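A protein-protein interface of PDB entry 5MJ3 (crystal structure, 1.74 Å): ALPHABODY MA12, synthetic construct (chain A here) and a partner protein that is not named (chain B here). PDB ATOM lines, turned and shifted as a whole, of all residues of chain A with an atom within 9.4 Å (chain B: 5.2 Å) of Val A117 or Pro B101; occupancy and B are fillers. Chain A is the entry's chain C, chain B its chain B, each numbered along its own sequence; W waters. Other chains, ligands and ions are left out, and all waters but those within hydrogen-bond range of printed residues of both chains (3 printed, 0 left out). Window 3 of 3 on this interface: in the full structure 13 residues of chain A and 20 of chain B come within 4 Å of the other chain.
The backbone carbonyl oxygen of Ala B28 is in hydrogen-bond range of the side-chain hydroxyl of Tyr A24 (3.2 Å).
The side-chain hydroxyl (OG) of Ser B100 lies close to the backbone NH (N) of Val B102 (3.5 Å). N of Gly B103 lies within hydrogen-bond range of OG of Ser B100, 3.1 Å away. The side-chain hydroxyl of Thr A118 sits at hydrogen-bond distance from the backbone carbonyl oxygen of Met A114, 2.7 Å away. NE2 of Gln B104 lies within hydrogen-bond range of O of Asp B99. The backbone carbonyl oxygen (O) of Tyr A24 is in hydrogen-bond range of the side-chain hydroxyl (OG1) of Thr A27 (2.6 Å).
Tyr A24 touches Ser B27. Pro B101 touches Val A117 (CD to O, 3.6 Å). CG2 of Thr A118 touches OD2 of Asp B99, at 3.6 Å. Thr A118 touches Ser B100.
Of the printed residues of chain B, Tyr A24 touches Ser B27 and Ala B28. Ile A48 touches none of the printed residues of chain B. Of chain B, only Pro B101 (3.6 Å) comes within 4 Å of Val A117. Printed residues of chain B within 4 Å of Thr A118: Asp B99 and Ser B100. Of the printed residues of chain A, Ser B27 touches Tyr A24 (3.4 Å). Ala B28 touches just one residue of chain A: Tyr A24 (3.2 Å). Of the printed residues of chain A, Asp B99 touches Thr A118. Of chain A, only Thr A118 comes within 4 Å of Ser B100. Pro B101 touches just one residue of chain A: Val A117. Gly B103 touches none of the printed residues of chain A. The nearest residue of chain B that does not touch Val A117 is Ser B100 (5.1 Å). The nearest residue of chain A that does not touch Pro B101 is Thr A118 (4.2 Å).
Of the 10 printed residues of chain B, 5 touch a printed residue of chain A. Hydrophobic or aromatic side chains of chain B that line the printed part of chain A: Pro B101. Of the 17 printed residues of chain A, 3 touch a printed residue of chain B. Hydrophobic or aromatic side chains of chain A within 4 Å of the printed part of chain B: Tyr A24 and Val A117. Among the printed residues, 5 pairs touch across the chains. Among the printed residues, no Asp or Glu carboxylate lies within 4 Å of a Lys or Arg side-chain nitrogen of the other chain.
Water W3 bridges OH of Tyr A24 and O of Ser B27. Water W1 bridges the backbone carbonyl oxygen of Ser B27 (2.8 Å) and the side-chain hydroxyl of Thr A27 (3.0 Å). Water W2 lies within hydrogen-bond range of N of Val B102, O of Ala B28 and SD of Met A114.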
ATOM      1  N   TYR A  24     -13.249  35.756 -14.772  1.00  0.00           N
ATOM      2  CA  TYR A  24     -12.247  34.710 -14.939  1.00  0.00           C
ATOM      3  C   TYR A  24     -10.855  35.307 -15.128  1.00  0.00           C
ATOM      4  O   TYR A  24      -9.867  34.781 -14.602  1.00  0.00           O
ATOM      5  CB  TYR A  24     -12.643  33.838 -16.128  1.00  0.00           C
ATOM      6  CG  TYR A  24     -11.764  32.641 -16.377  1.00  0.00           C
ATOM      7  CD1 TYR A  24     -11.860  31.500 -15.595  1.00  0.00           C
ATOM      8  CD2 TYR A  24     -10.840  32.651 -17.417  1.00  0.00           C
ATOM      9  CE1 TYR A  24     -11.046  30.391 -15.844  1.00  0.00           C
ATOM     10  CE2 TYR A  24     -10.044  31.571 -17.663  1.00  0.00           C
ATOM     11  CZ  TYR A  24     -10.147  30.447 -16.885  1.00  0.00           C
ATOM     12  OH  TYR A  24      -9.332  29.378 -17.165  1.00  0.00           O
ATOM     13  N   ILE A  25     -10.766  36.416 -15.867  1.00  0.00           N
ATOM     14  CA  ILE A  25      -9.484  37.085 -16.073  1.00  0.00           C
ATOM     15  C   ILE A  25      -8.879  37.528 -14.744  1.00  0.00           C
ATOM     16  O   ILE A  25      -7.660  37.476 -14.560  1.00  0.00           O
ATOM     17  CB  ILE A  25      -9.660  38.268 -17.042  1.00  0.00           C
ATOM     18  CG1 ILE A  25      -9.978  37.727 -18.436  1.00  0.00           C
ATOM     19  CG2 ILE A  25      -8.404  39.140 -17.066  1.00  0.00           C
ATOM     20  CD1 ILE A  25     -10.319  38.803 -19.443  1.00  0.00           C
ATOM     21  N   TYR A  26      -9.706  37.995 -13.808  1.00  0.00           N
ATOM     22  CA  TYR A  26      -9.179  38.346 -12.492  1.00  0.00           C
ATOM     23  C   TYR A  26      -8.454  37.169 -11.856  1.00  0.00           C
ATOM     24  O   TYR A  26      -7.363  37.331 -11.295  1.00  0.00           O
ATOM     25  CB  TYR A  26     -10.305  38.817 -11.572  1.00  0.00           C
ATOM     26  CG  TYR A  26     -10.996  40.088 -12.007  1.00  0.00           C
ATOM     27  CD1 TYR A  26     -10.349  41.029 -12.796  1.00  0.00           C
ATOM     28  CD2 TYR A  26     -12.303  40.348 -11.617  1.00  0.00           C
ATOM     29  CE1 TYR A  26     -10.985  42.190 -13.187  1.00  0.00           C
ATOM     30  CE2 TYR A  26     -12.947  41.501 -12.001  1.00  0.00           C
ATOM     31  CZ  TYR A  26     -12.286  42.420 -12.785  1.00  0.00           C
ATOM     32  OH  TYR A  26     -12.933  43.571 -13.169  1.00  0.00           O
ATOM     33  N   THR A  27      -9.039  35.973 -11.940  1.00  0.00           N
ATOM     34  CA  THR A  27      -8.449  34.793 -11.311  1.00  0.00           C
ATOM     35  C   THR A  27      -7.090  34.435 -11.900  1.00  0.00           C
ATOM     36  O   THR A  27      -6.371  33.629 -11.304  1.00  0.00           O
ATOM     37  CB  THR A  27      -9.395  33.583 -11.433  1.00  0.00           C
ATOM     38  OG1 THR A  27      -9.340  33.034 -12.761  1.00  0.00           O
ATOM     39  CG2 THR A  27     -10.848  33.963 -11.090  1.00  0.00           C
ATOM     40  N   MET A  28      -6.728  35.010 -13.044  1.00  0.00           N
ATOM     41  CA  MET A  28      -5.455  34.715 -13.696  1.00  0.00           C
ATOM     42  C   MET A  28      -4.585  35.968 -13.803  1.00  0.00           C
ATOM     43  O   MET A  28      -4.808  36.959 -13.100  1.00  0.00           O
ATOM     44  CB  MET A  28      -5.701  34.125 -15.089  1.00  0.00           C
ATOM     45  CG  MET A  28      -6.641  34.957 -15.950  1.00  0.00           C
ATOM     46  SD  MET A  28      -6.936  34.314 -17.615  1.00  0.00           S
ATOM     47  CE  MET A  28      -5.318  34.526 -18.356  1.00  0.00           C
ATOM     48  N   ILE A  48      -3.117  41.112 -21.021  1.00  0.00           N
ATOM     49  CA  ILE A  48      -4.337  41.005 -20.225  1.00  0.00           C
ATOM     50  C   ILE A  48      -5.066  42.341 -20.186  1.00  0.00           C
ATOM     51  O   ILE A  48      -6.291  42.403 -20.352  1.00  0.00           O
ATOM     52  CB  ILE A  48      -4.012  40.513 -18.804  1.00  0.00           C
ATOM     53  CG1 ILE A  48      -3.428  39.099 -18.845  1.00  0.00           C
ATOM     54  CG2 ILE A  48      -5.263  40.547 -17.930  1.00  0.00           C
ATOM     55  CD1 ILE A  48      -2.850  38.634 -17.518  1.00  0.00           C
ATOM     56  N   ILE A  51      -7.003  42.827 -23.322  1.00  0.00           N
ATOM     57  CA  ILE A  51      -8.208  42.009 -23.399  1.00  0.00           C
ATOM     58  C   ILE A  51      -9.299  42.576 -22.495  1.00  0.00           C
ATOM     59  O   ILE A  51     -10.483  42.573 -22.853  1.00  0.00           O
ATOM     60  CB  ILE A  51      -7.878  40.541 -23.052  1.00  0.00           C
ATOM     61  CG1 ILE A  51      -7.002  39.934 -24.152  1.00  0.00           C
ATOM     62  CG2 ILE A  51      -9.156  39.733 -22.892  1.00  0.00           C
ATOM     63  CD1 ILE A  51      -6.531  38.521 -23.883  1.00  0.00           C
ATOM     64  N   ILE A 109     -11.990  36.454 -28.142  1.00  0.00           N
ATOM     65  CA  ILE A 109     -11.412  36.731 -26.823  1.00  0.00           C
ATOM     66  C   ILE A 109     -11.315  35.449 -26.006  1.00  0.00           C
ATOM     67  O   ILE A 109     -10.298  35.173 -25.360  1.00  0.00           O
ATOM     68  CB  ILE A 109     -12.253  37.789 -26.080  1.00  0.00           C
ATOM     69  CG1 ILE A 109     -12.139  39.144 -26.771  1.00  0.00           C
ATOM     70  CG2 ILE A 109     -11.847  37.870 -24.596  1.00  0.00           C
ATOM     71  CD1 ILE A 109     -13.141  40.164 -26.279  1.00  0.00           C
ATOM     72  N   TYR A 110     -12.408  34.688 -25.962  1.00  0.00           N
ATOM     73  CA  TYR A 110     -12.416  33.414 -25.260  1.00  0.00           C
ATOM     74  C   TYR A 110     -11.278  32.515 -25.736  1.00  0.00           C
ATOM     75  O   TYR A 110     -10.550  31.926 -24.930  1.00  0.00           O
ATOM     76  CB  TYR A 110     -13.777  32.750 -25.468  1.00  0.00           C
ATOM     77  CG  TYR A 110     -13.918  31.349 -24.915  1.00  0.00           C
ATOM     78  CD1 TYR A 110     -14.375  31.126 -23.621  1.00  0.00           C
ATOM     79  CD2 TYR A 110     -13.637  30.249 -25.705  1.00  0.00           C
ATOM     80  CE1 TYR A 110     -14.529  29.830 -23.119  1.00  0.00           C
ATOM     81  CE2 TYR A 110     -13.772  28.967 -25.218  1.00  0.00           C
ATOM     82  CZ  TYR A 110     -14.230  28.762 -23.937  1.00  0.00           C
ATOM     83  OH  TYR A 110     -14.379  27.479 -23.493  1.00  0.00           O
ATOM     84  N   LYS A 111     -11.093  32.413 -27.050  1.00  0.00           N
ATOM     85  CA  LYS A 111     -10.012  31.573 -27.558  1.00  0.00           C
ATOM     86  C   LYS A 111      -8.651  32.099 -27.122  1.00  0.00           C
ATOM     87  O   LYS A 111      -7.761  31.314 -26.785  1.00  0.00           O
ATOM     88  CB  LYS A 111     -10.096  31.455 -29.078  1.00  0.00           C
ATOM     89  CG  LYS A 111     -11.221  30.522 -29.524  1.00  0.00           C
ATOM     90  CD  LYS A 111     -11.145  30.155 -31.001  1.00  0.00           C
ATOM     91  CE  LYS A 111     -11.480  31.309 -31.917  1.00  0.00           C
ATOM     92  NZ  LYS A 111     -11.631  30.844 -33.334  1.00  0.00           N
ATOM     93  N   GLN A 112      -8.463  33.421 -27.121  1.00  0.00           N
ATOM     94  CA  GLN A 112      -7.196  33.975 -26.640  1.00  0.00           C
ATOM     95  C   GLN A 112      -6.946  33.609 -25.182  1.00  0.00           C
ATOM     96  O   GLN A 112      -5.838  33.212 -24.808  1.00  0.00           O
ATOM     97  CB  GLN A 112      -7.179  35.497 -26.801  1.00  0.00           C
ATOM     98  CG  GLN A 112      -6.937  35.977 -28.217  1.00  0.00           C
ATOM     99  CD  GLN A 112      -6.625  37.462 -28.291  1.00  0.00           C
ATOM    100  OE1 GLN A 112      -6.953  38.228 -27.384  1.00  0.00           O
ATOM    101  NE2 GLN A 112      -5.982  37.874 -29.376  1.00  0.00           N
ATOM    102  N   ILE A 113      -7.962  33.773 -24.333  1.00  0.00           N
ATOM    103  CA  ILE A 113      -7.811  33.471 -22.908  1.00  0.00           C
ATOM    104  C   ILE A 113      -7.546  31.989 -22.693  1.00  0.00           C
ATOM    105  O   ILE A 113      -6.695  31.603 -21.886  1.00  0.00           O
ATOM    106  CB  ILE A 113      -9.065  33.923 -22.131  1.00  0.00           C
ATOM    107  CG1 ILE A 113      -9.218  35.446 -22.201  1.00  0.00           C
ATOM    108  CG2 ILE A 113      -8.995  33.458 -20.690  1.00  0.00           C
ATOM    109  CD1 ILE A 113      -8.127  36.211 -21.490  1.00  0.00           C
ATOM    110  N   MET A 114      -8.305  31.128 -23.373  1.00  0.00           N
ATOM    111  CA  MET A 114      -8.078  29.696 -23.200  1.00  0.00           C
ATOM    112  C   MET A 114      -6.668  29.314 -23.628  1.00  0.00           C
ATOM    113  O   MET A 114      -6.035  28.441 -23.017  1.00  0.00           O
ATOM    114  CB  MET A 114      -9.114  28.891 -23.988  1.00  0.00           C
ATOM    115  CG  MET A 114     -10.514  28.867 -23.376  1.00  0.00           C
ATOM    116  SD  MET A 114     -10.553  28.308 -21.650  1.00  0.00           S
ATOM    117  CE  MET A 114     -10.780  29.878 -20.840  1.00  0.00           C
ATOM    118  N   ALA A 115      -6.152  29.944 -24.681  1.00  0.00           N
ATOM    119  CA  ALA A 115      -4.780  29.649 -25.088  1.00  0.00           C
ATOM    120  C   ALA A 115      -3.784  30.142 -24.045  1.00  0.00           C
ATOM    121  O   ALA A 115      -2.742  29.512 -23.830  1.00  0.00           O
ATOM    122  CB  ALA A 115      -4.492  30.270 -26.451  1.00  0.00           C
ATOM    123  N   MET A 116      -4.104  31.240 -23.356  1.00  0.00           N
ATOM    124  CA  MET A 116      -3.191  31.789 -22.360  1.00  0.00           C
ATOM    125  C   MET A 116      -3.095  30.914 -21.119  1.00  0.00           C
ATOM    126  O   MET A 116      -2.032  30.853 -20.493  1.00  0.00           O
ATOM    127  CB  MET A 116      -3.632  33.197 -21.965  1.00  0.00           C
ATOM    128  CG  MET A 116      -3.327  34.245 -23.009  1.00  0.00           C
ATOM    129  SD  MET A 116      -4.138  35.819 -22.672  1.00  0.00           S
ATOM    130  CE  MET A 116      -3.486  36.212 -21.055  1.00  0.00           C
ATOM    131  N   VAL A 117      -4.186  30.240 -20.732  1.00  0.00           N
ATOM    132  CA  VAL A 117      -4.159  29.382 -19.548  1.00  0.00           C
ATOM    133  C   VAL A 117      -3.801  27.939 -19.880  1.00  0.00           C
ATOM    134  O   VAL A 117      -3.751  27.098 -18.970  1.00  0.00           O
ATOM    135  CB  VAL A 117      -5.504  29.419 -18.790  1.00  0.00           C
ATOM    136  CG1 VAL A 117      -5.877  30.843 -18.428  1.00  0.00           C
ATOM    137  CG2 VAL A 117      -6.607  28.786 -19.604  1.00  0.00           C
ATOM    138  N   THR A 118      -3.550  27.622 -21.145  1.00  0.00           N
ATOM    139  CA  THR A 118      -3.117  26.279 -21.527  1.00  0.00           C
ATOM    140  C   THR A 118      -1.607  26.248 -21.760  1.00  0.00           C
ATOM    141  O   THR A 118      -1.009  27.205 -22.259  1.00  0.00           O
ATOM    142  CB  THR A 118      -3.831  25.786 -22.801  1.00  0.00           C
ATOM    143  OG1 THR A 118      -5.250  25.896 -22.626  1.00  0.00           O
ATOM    144  CG2 THR A 118      -3.467  24.326 -23.096  1.00  0.00           C
ATOM    145  OXT THR A 118      -0.953  25.248 -21.456  1.00  0.00           O
ATOM    146  N   SER B  27     -12.595  26.442 -10.972  1.00  0.00           N
ATOM    147  CA  SER B  27     -11.510  27.300 -11.447  1.00  0.00           C
ATOM    148  C   SER B  27     -11.146  27.085 -12.915  1.00  0.00           C
ATOM    149  O   SER B  27     -10.491  27.953 -13.505  1.00  0.00           O
ATOM    150  CB  SER B  27     -10.247  27.081 -10.598  1.00  0.00           C
ATOM    151  OG  SER B  27      -9.726  25.790 -10.821  1.00  0.00           O
ATOM    152  N   ALA B  28     -11.551  25.967 -13.525  1.00  0.00           N
ATOM    153  CA  ALA B  28     -11.031  25.620 -14.846  1.00  0.00           C
ATOM    154  C   ALA B  28     -11.563  26.493 -15.978  1.00  0.00           C
ATOM    155  O   ALA B  28     -10.930  26.570 -17.028  1.00  0.00           O
ATOM    156  CB  ALA B  28     -11.342  24.157 -15.167  1.00  0.00           C
ATOM    157  N   ASP B  99      -4.569  19.504 -22.554  1.00  0.00           N
ATOM    158  CA  ASP B  99      -3.756  20.044 -21.471  1.00  0.00           C
ATOM    159  C   ASP B  99      -4.334  21.325 -20.874  1.00  0.00           C
ATOM    160  O   ASP B  99      -3.698  21.923 -20.000  1.00  0.00           O
ATOM    161  CB  ASP B  99      -2.299  20.284 -21.942  1.00  0.00           C
ATOM    162  CG  ASP B  99      -2.185  20.702 -23.425  1.00  0.00           C
ATOM    163  OD1 ASP B  99      -2.924  20.168 -24.284  1.00  0.00           O
ATOM    164  OD2 ASP B  99      -1.315  21.547 -23.736  1.00  0.00           O
ATOM    165  N   SER B 100      -5.518  21.752 -21.311  1.00  0.00           N
ATOM    166  CA  SER B 100      -6.149  22.934 -20.746  1.00  0.00           C
ATOM    167  C   SER B 100      -6.646  22.626 -19.332  1.00  0.00           C
ATOM    168  O   SER B 100      -6.702  21.464 -18.916  1.00  0.00           O
ATOM    169  CB  SER B 100      -7.311  23.397 -21.626  1.00  0.00           C
ATOM    170  OG  SER B 100      -8.383  22.470 -21.590  1.00  0.00           O
ATOM    171  N   PRO B 101      -6.998  23.653 -18.564  1.00  0.00           N
ATOM    172  CA  PRO B 101      -7.638  23.401 -17.256  1.00  0.00           C
ATOM    173  C   PRO B 101      -8.837  22.475 -17.338  1.00  0.00           C
ATOM    174  O   PRO B 101      -9.009  21.613 -16.466  1.00  0.00           O
ATOM    175  CB  PRO B 101      -8.038  24.808 -16.794  1.00  0.00           C
ATOM    176  CG  PRO B 101      -7.050  25.713 -17.463  1.00  0.00           C
ATOM    177  CD  PRO B 101      -6.778  25.089 -18.806  1.00  0.00           C
ATOM    178  N   VAL B 102      -9.681  22.628 -18.358  1.00  0.00           N
ATOM    179  CA  VAL B 102     -10.790  21.692 -18.533  1.00  0.00           C
ATOM    180  C   VAL B 102     -10.265  20.292 -18.840  1.00  0.00           C
ATOM    181  O   VAL B 102     -10.865  19.295 -18.423  1.00  0.00           O
ATOM    182  CB  VAL B 102     -11.759  22.182 -19.624  1.00  0.00           C
ATOM    183  CG1 VAL B 102     -12.822  21.127 -19.932  1.00  0.00           C
ATOM    184  CG2 VAL B 102     -12.457  23.456 -19.166  1.00  0.00           C
ATOM    185  N   GLY B 103      -9.160  20.197 -19.574  1.00  0.00           N
ATOM    186  CA  GLY B 103      -8.536  18.900 -19.805  1.00  0.00           C
ATOM    187  C   GLY B 103      -8.005  18.272 -18.526  1.00  0.00           C
ATOM    188  O   GLY B 103      -8.058  17.051 -18.352  1.00  0.00           O
ATOM    189  N   GLN B 104      -7.474  19.098 -17.621  1.00  0.00           N
ATOM    190  CA  GLN B 104      -7.037  18.622 -16.313  1.00  0.00           C
ATOM    191  C   GLN B 104      -8.223  18.176 -15.463  1.00  0.00           C
ATOM    192  O   GLN B 104      -8.115  17.229 -14.672  1.00  0.00           O
ATOM    193  CB  GLN B 104      -6.264  19.724 -15.592  1.00  0.00           C
ATOM    194  CG  GLN B 104      -4.936  20.099 -16.237  1.00  0.00           C
ATOM    195  CD  GLN B 104      -4.356  21.380 -15.663  1.00  0.00           C
ATOM    196  OE1 GLN B 104      -4.449  21.635 -14.463  1.00  0.00           O
ATOM    197  NE2 GLN B 104      -3.769  22.202 -16.528  1.00  0.00           N
ATOM    198  N   LEU B 105      -9.346  18.884 -15.576  1.00  0.00           N
ATOM    199  CA  LEU B 105     -10.561  18.478 -14.886  1.00  0.00           C
ATOM    200  C   LEU B 105     -11.034  17.111 -15.375  1.00  0.00           C
ATOM    201  O   LEU B 105     -11.421  16.252 -14.572  1.00  0.00           O
ATOM    202  CB  LEU B 105     -11.625  19.554 -15.094  1.00  0.00           C
ATOM    203  CG  LEU B 105     -13.028  19.297 -14.547  1.00  0.00           C
ATOM    204  CD1 LEU B 105     -12.987  19.106 -13.051  1.00  0.00           C
ATOM    205  CD2 LEU B 105     -13.928  20.475 -14.931  1.00  0.00           C
ATOM    206  N   HIS B 106     -10.972  16.887 -16.688  1.00  0.00           N
ATOM    207  CA  HIS B 106     -11.315  15.587 -17.254  1.00  0.00           C
ATOM    208  C   HIS B 106     -10.404  14.499 -16.690  1.00  0.00           C
ATOM    209  O   HIS B 106     -10.873  13.426 -16.291  1.00  0.00           O
ATOM    210  CB  HIS B 106     -11.203  15.662 -18.776  1.00  0.00           C
ATOM    211  CG  HIS B 106     -11.449  14.366 -19.483  1.00  0.00           C
ATOM    212  ND1 HIS B 106     -10.446  13.452 -19.736  1.00  0.00           N
ATOM    213  CD2 HIS B 106     -12.574  13.853 -20.032  1.00  0.00           C
ATOM    214  CE1 HIS B 106     -10.950  12.421 -20.392  1.00  0.00           C
ATOM    215  NE2 HIS B 106     -12.240  12.640 -20.584  1.00  0.00           N
HETATM  216  O   HOH W   1     -10.657  30.440 -12.232  1.00  0.00           O
HETATM  217  O   HOH W   2      -9.929  25.330 -19.762  1.00  0.00           O
HETATM  218  O   HOH W   3      -8.192  28.464 -15.111  1.00  0.00           O
